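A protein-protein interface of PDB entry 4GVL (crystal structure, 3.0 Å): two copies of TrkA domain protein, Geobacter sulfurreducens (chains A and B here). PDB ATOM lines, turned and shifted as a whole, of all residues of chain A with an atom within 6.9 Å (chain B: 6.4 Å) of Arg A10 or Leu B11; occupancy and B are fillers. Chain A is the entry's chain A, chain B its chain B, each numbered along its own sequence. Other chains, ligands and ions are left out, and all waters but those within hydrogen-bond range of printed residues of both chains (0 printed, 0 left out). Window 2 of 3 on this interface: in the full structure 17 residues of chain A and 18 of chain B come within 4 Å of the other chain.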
ATOM      1  N   PRO A   5       4.495  -6.874   3.469  1.00  0.00           N
ATOM      2  CA  PRO A   5       4.370  -5.449   3.085  1.00  0.00           C
ATOM      3  C   PRO A   5       4.662  -5.123   1.622  1.00  0.00           C
ATOM      4  O   PRO A   5       4.067  -4.197   1.070  1.00  0.00           O
ATOM      5  CB  PRO A   5       5.389  -4.746   3.992  1.00  0.00           C
ATOM      6  CG  PRO A   5       6.370  -5.816   4.366  1.00  0.00           C
ATOM      7  CD  PRO A   5       5.560  -7.074   4.473  1.00  0.00           C
ATOM      8  N   TRP A   6       5.573  -5.869   1.006  1.00  0.00           N
ATOM      9  CA  TRP A   6       5.924  -5.647  -0.393  1.00  0.00           C
ATOM     10  C   TRP A   6       5.025  -6.435  -1.361  1.00  0.00           C
ATOM     11  O   TRP A   6       4.948  -6.102  -2.547  1.00  0.00           O
ATOM     12  CB  TRP A   6       7.410  -5.943  -0.627  1.00  0.00           C
ATOM     13  CG  TRP A   6       7.773  -6.128  -2.072  1.00  0.00           C
ATOM     14  CD1 TRP A   6       8.052  -5.148  -2.986  1.00  0.00           C
ATOM     15  CD2 TRP A   6       7.883  -7.378  -2.772  1.00  0.00           C
ATOM     16  NE1 TRP A   6       8.336  -5.711  -4.212  1.00  0.00           N
ATOM     17  CE2 TRP A   6       8.237  -7.076  -4.110  1.00  0.00           C
ATOM     18  CE3 TRP A   6       7.718  -8.724  -2.397  1.00  0.00           C
ATOM     19  CZ2 TRP A   6       8.431  -8.075  -5.076  1.00  0.00           C
ATOM     20  CZ3 TRP A   6       7.912  -9.717  -3.359  1.00  0.00           C
ATOM     21  CH2 TRP A   6       8.266  -9.386  -4.682  1.00  0.00           C
ATOM     22  N   ILE A   7       4.349  -7.467  -0.860  1.00  0.00           N
ATOM     23  CA  ILE A   7       3.376  -8.202  -1.673  1.00  0.00           C
ATOM     24  C   ILE A   7       2.010  -7.495  -1.675  1.00  0.00           C
ATOM     25  O   ILE A   7       1.330  -7.449  -2.703  1.00  0.00           O
ATOM     26  CB  ILE A   7       3.250  -9.680  -1.245  1.00  0.00           C
ATOM     27  CG1 ILE A   7       4.644 -10.313  -1.146  1.00  0.00           C
ATOM     28  CG2 ILE A   7       2.392 -10.453  -2.248  1.00  0.00           C
ATOM     29  CD1 ILE A   7       4.690 -11.662  -0.456  1.00  0.00           C
ATOM     30  N   GLU A   8       1.628  -6.930  -0.529  1.00  0.00           N
ATOM     31  CA  GLU A   8       0.404  -6.123  -0.419  1.00  0.00           C
ATOM     32  C   GLU A   8       0.469  -4.926  -1.363  1.00  0.00           C
ATOM     33  O   GLU A   8      -0.558  -4.398  -1.790  1.00  0.00           O
ATOM     34  CB  GLU A   8       0.169  -5.658   1.031  1.00  0.00           C
ATOM     35  CG  GLU A   8      -0.800  -6.536   1.871  1.00  0.00           C
ATOM     36  CD  GLU A   8      -0.129  -7.724   2.596  1.00  0.00           C
ATOM     37  OE1 GLU A   8       0.359  -8.659   1.920  1.00  0.00           O
ATOM     38  OE2 GLU A   8      -0.119  -7.735   3.849  1.00  0.00           O
ATOM     39  N   ARG A   9       1.694  -4.517  -1.678  1.00  0.00           N
ATOM     40  CA  ARG A   9       1.983  -3.466  -2.647  1.00  0.00           C
ATOM     41  C   ARG A   9       1.565  -3.875  -4.065  1.00  0.00           C
ATOM     42  O   ARG A   9       1.064  -3.058  -4.830  1.00  0.00           O
ATOM     43  CB  ARG A   9       3.480  -3.166  -2.610  1.00  0.00           C
ATOM     44  CG  ARG A   9       3.946  -2.048  -3.511  1.00  0.00           C
ATOM     45  CD  ARG A   9       5.187  -2.487  -4.260  1.00  0.00           C
ATOM     46  NE  ARG A   9       5.975  -1.355  -4.736  1.00  0.00           N
ATOM     47  CZ  ARG A   9       6.848  -1.414  -5.737  1.00  0.00           C
ATOM     48  NH1 ARG A   9       7.520  -0.329  -6.087  1.00  0.00           N
ATOM     49  NH2 ARG A   9       7.050  -2.548  -6.395  1.00  0.00           N
ATOM     50  N   ARG A  10       1.760  -5.146  -4.401  1.00  0.00           N
ATOM     51  CA  ARG A  10       1.465  -5.651  -5.741  1.00  0.00           C
ATOM     52  C   ARG A  10       0.016  -6.094  -5.932  1.00  0.00           C
ATOM     53  O   ARG A  10      -0.373  -6.509  -7.025  1.00  0.00           O
ATOM     54  CB  ARG A  10       2.412  -6.803  -6.101  1.00  0.00           C
ATOM     55  CG  ARG A  10       3.835  -6.377  -6.429  1.00  0.00           C
ATOM     56  CD  ARG A  10       3.884  -5.575  -7.712  1.00  0.00           C
ATOM     57  NE  ARG A  10       5.248  -5.421  -8.204  1.00  0.00           N
ATOM     58  CZ  ARG A  10       5.599  -4.620  -9.206  1.00  0.00           C
ATOM     59  NH1 ARG A  10       4.686  -3.883  -9.829  1.00  0.00           N
ATOM     60  NH2 ARG A  10       6.868  -4.549  -9.582  1.00  0.00           N
ATOM     61  N   LEU A  11      -0.777  -6.018  -4.870  1.00  0.00           N
ATOM     62  CA  LEU A  11      -2.196  -6.330  -4.967  1.00  0.00           C
ATOM     63  C   LEU A  11      -3.002  -5.068  -5.250  1.00  0.00           C
ATOM     64  O   LEU A  11      -2.439  -3.971  -5.327  1.00  0.00           O
ATOM     65  CB  LEU A  11      -2.691  -7.015  -3.694  1.00  0.00           C
ATOM     66  CG  LEU A  11      -2.222  -8.448  -3.431  1.00  0.00           C
ATOM     67  CD1 LEU A  11      -2.776  -8.922  -2.103  1.00  0.00           C
ATOM     68  CD2 LEU A  11      -2.622  -9.406  -4.555  1.00  0.00           C
ATOM     69  N   ARG A  12      -4.316  -5.227  -5.409  1.00  0.00           N
ATOM     70  CA  ARG A  12      -5.202  -4.096  -5.668  1.00  0.00           C
ATOM     71  C   ARG A  12      -5.147  -3.108  -4.518  1.00  0.00           C
ATOM     72  O   ARG A  12      -5.028  -3.500  -3.357  1.00  0.00           O
ATOM     73  CB  ARG A  12      -6.644  -4.549  -5.872  1.00  0.00           C
ATOM     74  CG  ARG A  12      -7.431  -3.613  -6.779  1.00  0.00           C
ATOM     75  CD  ARG A  12      -8.817  -3.296  -6.242  1.00  0.00           C
ATOM     76  NE  ARG A  12      -9.629  -4.493  -6.056  1.00  0.00           N
ATOM     77  CZ  ARG A  12     -10.937  -4.484  -5.815  1.00  0.00           C
ATOM     78  NH1 ARG A  12     -11.592  -3.328  -5.735  1.00  0.00           N
ATOM     79  NH2 ARG A  12     -11.589  -5.637  -5.653  1.00  0.00           N
ATOM     80  N   TYR A  13      -5.241  -1.826  -4.842  1.00  0.00           N
ATOM     81  CA  TYR A  13      -5.060  -0.804  -3.837  1.00  0.00           C
ATOM     82  C   TYR A  13      -6.288  -0.566  -2.974  1.00  0.00           C
ATOM     83  O   TYR A  13      -7.394  -0.360  -3.476  1.00  0.00           O
ATOM     84  CB  TYR A  13      -4.606   0.503  -4.466  1.00  0.00           C
ATOM     85  CG  TYR A  13      -4.329   1.568  -3.443  1.00  0.00           C
ATOM     86  CD1 TYR A  13      -3.355   1.382  -2.467  1.00  0.00           C
ATOM     87  CD2 TYR A  13      -5.041   2.762  -3.441  1.00  0.00           C
ATOM     88  CE1 TYR A  13      -3.095   2.361  -1.515  1.00  0.00           C
ATOM     89  CE2 TYR A  13      -4.787   3.753  -2.491  1.00  0.00           C
ATOM     90  CZ  TYR A  13      -3.809   3.546  -1.535  1.00  0.00           C
ATOM     91  OH  TYR A  13      -3.543   4.515  -0.596  1.00  0.00           O
ATOM     92  N   ILE B   7       5.180 -13.183 -15.871  1.00  0.00           N
ATOM     93  CA  ILE B   7       4.317 -13.541 -14.747  1.00  0.00           C
ATOM     94  C   ILE B   7       4.066 -12.289 -13.908  1.00  0.00           C
ATOM     95  O   ILE B   7       2.927 -11.990 -13.541  1.00  0.00           O
ATOM     96  CB  ILE B   7       4.944 -14.657 -13.846  1.00  0.00           C
ATOM     97  CG1 ILE B   7       5.312 -15.909 -14.656  1.00  0.00           C
ATOM     98  CG2 ILE B   7       3.996 -15.045 -12.712  1.00  0.00           C
ATOM     99  CD1 ILE B   7       6.795 -16.060 -14.938  1.00  0.00           C
ATOM    100  N   GLU B   8       5.145 -11.552 -13.651  1.00  0.00           N
ATOM    101  CA  GLU B   8       5.129 -10.360 -12.807  1.00  0.00           C
ATOM    102  C   GLU B   8       4.051  -9.327 -13.172  1.00  0.00           C
ATOM    103  O   GLU B   8       3.140  -9.093 -12.380  1.00  0.00           O
ATOM    104  CB  GLU B   8       6.538  -9.739 -12.753  1.00  0.00           C
ATOM    105  CG  GLU B   8       6.661  -8.403 -12.035  1.00  0.00           C
ATOM    106  CD  GLU B   8       6.530  -7.227 -12.978  1.00  0.00           C
ATOM    107  OE1 GLU B   8       7.307  -7.149 -13.959  1.00  0.00           O
ATOM    108  OE2 GLU B   8       5.644  -6.384 -12.736  1.00  0.00           O
ATOM    109  N   ARG B   9       4.138  -8.752 -14.373  1.00  0.00           N
ATOM    110  CA  ARG B   9       3.320  -7.587 -14.777  1.00  0.00           C
ATOM    111  C   ARG B   9       1.792  -7.816 -14.917  1.00  0.00           C
ATOM    112  O   ARG B   9       1.045  -6.901 -15.270  1.00  0.00           O
ATOM    113  CB  ARG B   9       3.951  -6.905 -16.010  1.00  0.00           C
ATOM    114  CG  ARG B   9       3.102  -6.837 -17.279  1.00  0.00           C
ATOM    115  CD  ARG B   9       3.076  -8.173 -18.026  1.00  0.00           C
ATOM    116  NE  ARG B   9       2.292  -8.077 -19.254  1.00  0.00           N
ATOM    117  CZ  ARG B   9       1.889  -9.115 -19.978  1.00  0.00           C
ATOM    118  NH1 ARG B   9       1.176  -8.904 -21.077  1.00  0.00           N
ATOM    119  NH2 ARG B   9       2.189 -10.356 -19.610  1.00  0.00           N
ATOM    120  N   ARG B  10       1.344  -9.035 -14.620  1.00  0.00           N
ATOM    121  CA  ARG B  10      -0.084  -9.350 -14.516  1.00  0.00           C
ATOM    122  C   ARG B  10      -0.666  -8.878 -13.184  1.00  0.00           C
ATOM    123  O   ARG B  10      -1.864  -9.006 -12.941  1.00  0.00           O
ATOM    124  CB  ARG B  10      -0.308 -10.859 -14.670  1.00  0.00           C
ATOM    125  CG  ARG B  10      -0.336 -11.368 -16.106  1.00  0.00           C
ATOM    126  CD  ARG B  10      -1.554 -10.836 -16.849  1.00  0.00           C
ATOM    127  NE  ARG B  10      -1.908 -11.655 -18.009  1.00  0.00           N
ATOM    128  CZ  ARG B  10      -2.837 -11.324 -18.903  1.00  0.00           C
ATOM    129  NH1 ARG B  10      -3.511 -10.186 -18.783  1.00  0.00           N
ATOM    130  NH2 ARG B  10      -3.093 -12.132 -19.923  1.00  0.00           N
ATOM    131  N   LEU B  11       0.199  -8.354 -12.320  1.00  0.00           N
ATOM    132  CA  LEU B  11      -0.199  -7.787 -11.037  1.00  0.00           C
ATOM    133  C   LEU B  11      -0.244  -6.266 -11.130  1.00  0.00           C
ATOM    134  O   LEU B  11       0.119  -5.686 -12.156  1.00  0.00           O
ATOM    135  CB  LEU B  11       0.781  -8.203  -9.938  1.00  0.00           C
ATOM    136  CG  LEU B  11       1.172  -9.673  -9.792  1.00  0.00           C
ATOM    137  CD1 LEU B  11       2.495  -9.770  -9.067  1.00  0.00           C
ATOM    138  CD2 LEU B  11       0.093 -10.494  -9.081  1.00  0.00           C
ATOM    139  N   ARG B  12      -0.677  -5.624 -10.049  1.00  0.00           N
ATOM    140  CA  ARG B  12      -0.816  -4.172 -10.014  1.00  0.00           C
ATOM    141  C   ARG B  12       0.470  -3.469 -10.450  1.00  0.00           C
ATOM    142  O   ARG B  12       1.561  -3.797  -9.980  1.00  0.00           O
ATOM    143  CB  ARG B  12      -1.263  -3.714  -8.626  1.00  0.00           C
ATOM    144  CG  ARG B  12      -2.024  -2.408  -8.626  1.00  0.00           C
ATOM    145  CD  ARG B  12      -1.255  -1.323  -7.921  1.00  0.00           C
ATOM    146  NE  ARG B  12      -1.377  -1.457  -6.473  1.00  0.00           N
ATOM    147  CZ  ARG B  12      -1.007  -0.527  -5.598  1.00  0.00           C
ATOM    148  NH1 ARG B  12      -0.485   0.626  -6.011  1.00  0.00           N
ATOM    149  NH2 ARG B  12      -1.166  -0.752  -4.303  1.00  0.00           N
ATOM    150  N   TYR B  13       0.325  -2.515 -11.365  1.00  0.00           N
ATOM    151  CA  TYR B  13       1.467  -1.863 -11.999  1.00  0.00           C
ATOM    152  C   TYR B  13       2.159  -0.834 -11.110  1.00  0.00           C
ATOM    153  O   TYR B  13       1.507  -0.026 -10.446  1.00  0.00           O
ATOM    154  CB  TYR B  13       1.047  -1.210 -13.327  1.00  0.00           C
ATOM    155  CG  TYR B  13       2.066  -0.238 -13.893  1.00  0.00           C
ATOM    156  CD1 TYR B  13       3.145  -0.691 -14.654  1.00  0.00           C
ATOM    157  CD2 TYR B  13       1.954   1.132 -13.657  1.00  0.00           C
ATOM    158  CE1 TYR B  13       4.089   0.199 -15.171  1.00  0.00           C
ATOM    159  CE2 TYR B  13       2.895   2.030 -14.165  1.00  0.00           C
ATOM    160  CZ  TYR B  13       3.956   1.558 -14.920  1.00  0.00           C
ATOM    161  OH  TYR B  13       4.881   2.445 -15.424  1.00  0.00           O
ATOM    162  N   HIS B  14       3.489  -0.869 -11.122  1.00  0.00           N
ATOM    163  CA  HIS B  14       4.297   0.176 -10.514  1.00  0.00           C
ATOM    164  C   HIS B  14       5.361   0.619 -11.493  1.00  0.00           C
ATOM    165  O   HIS B  14       5.959  -0.212 -12.171  1.00  0.00           O
ATOM    166  CB  HIS B  14       4.952  -0.321  -9.237  1.00  0.00           C
ATOM    167  CG  HIS B  14       3.984  -0.587  -8.133  1.00  0.00           C
ATOM    168  ND1 HIS B  14       3.222  -1.735  -8.074  1.00  0.00           N
ATOM    169  CD2 HIS B  14       3.647   0.147  -7.048  1.00  0.00           C
ATOM    170  CE1 HIS B  14       2.458  -1.698  -6.999  1.00  0.00           C
ATOM    171  NE2 HIS B  14       2.698  -0.568  -6.358  1.00  0.00           N
ATOM    172  N   PRO B  15       5.612   1.931 -11.564  1.00  0.00           N
ATOM    173  CA  PRO B  15       6.573   2.442 -12.526  1.00  0.00           C
ATOM    174  C   PRO B  15       7.996   2.342 -12.004  1.00  0.00           C
ATOM    175  O   PRO B  15       8.202   2.132 -10.807  1.00  0.00           O
ATOM    176  CB  PRO B  15       6.172   3.908 -12.657  1.00  0.00           C
ATOM    177  CG  PRO B  15       5.618   4.262 -11.325  1.00  0.00           C
ATOM    178  CD  PRO B  15       5.026   3.005 -10.741  1.00  0.00           C
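O of Leu A11 is in hydrogen-bond range of NE of Arg B12, 3.0 Å away. The guanidinium group of Arg A10 lies within salt-bridge range of the side-chain carboxylate of Glu B8 (3.8 Å). The backbone carbonyl oxygen (O) of Arg A9 is in hydrogen-bond range of the guanidinium group (NH2) of Arg B12 (3.3 Å). NH1 of Arg A10 is in hydrogen-bond range of ND1 of His B14, at 3.1 Å. The backbone carbonyl oxygen (O) of Arg A9 sits close to a ring nitrogen (NE2) of His B14, at 3.3 Å. The backbone carbonyl oxygen (O) of Arg B12 is in hydrogen-bond range of the guanidinium group (NH1) of Arg A10, at 3.1 Å.
The backbone carbonyl oxygen (O) of Arg B12 lies within hydrogen-bond range of a ring nitrogen (ND1) of His B14, 3.3 Å away.
O of Arg A10 touches CB of Leu B11, 3.6 Å away. Tyr A13 touches Arg B12 (CD1 to NH2, 3.6 Å).
Arg A10 touches just these residues of chain B: Glu B8, Leu B11, Arg B12 and His B14. Leu B11 touches one residue of chain A. Of the printed residues of chain A, Arg B12 touches Arg A9, Arg A10, Leu A11 and Tyr A13. Printed residues of chain B within 4 Å of Leu A11: Arg B12 (3.0 Å). Of the printed residues of chain B, Tyr A13 touches Arg B12. Of the printed residues of chain A, Glu B8 touches Arg A10. Printed residues of chain B within 4 Å of Arg A9: Arg B12 (3.3 Å) and His B14 (2.9 Å). The nearest residue of chain B that does not touch Arg A10 is Tyr B13 (4.2 Å). The nearest residue of chain A that does not touch Leu B11 is Leu A11 (5.4 Å). The nearest printed residue of chain A that does not touch Glu B8 is Trp A6 (7.2 Å).
Of the 9 printed residues of chain A, 4 touch a printed residue of chain B. Printed residues of chain A that touch a printed residue of chain B: Arg A9, Arg A10, Leu A11 and Tyr A13. Along chain A the printed residues that touch a printed residue of chain B span positions 9 to 13. Hydrophobic or aromatic side chains of chain B within 4 Å of the printed part of chain A: Leu B11 and His B14. Among the printed residues, Asp or Glu carboxylates within 4 Å of a Lys or Arg side-chain nitrogen of the other chain: Arg A10 with Glu B8 (3.8 Å).
Arg A9 touches Arg B12, but with the chains exchanged Arg A12 does not touch Arg B9 (11.3 Å). Arg A10 touches Glu B8, but with the chains exchanged Glu A8 does not touch Arg B10 (12.1 Å). Arg A10 touches Leu B11, but with the chains exchanged Leu A11 does not touch Arg B10 (8.4 Å). Tyr A13 touches Arg B12, but with the chains exchanged Arg A12 does not touch Tyr B13 (8.0 Å). Positions printed for both chains: 7, 8, 9, 10, 11, 12 and 13.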
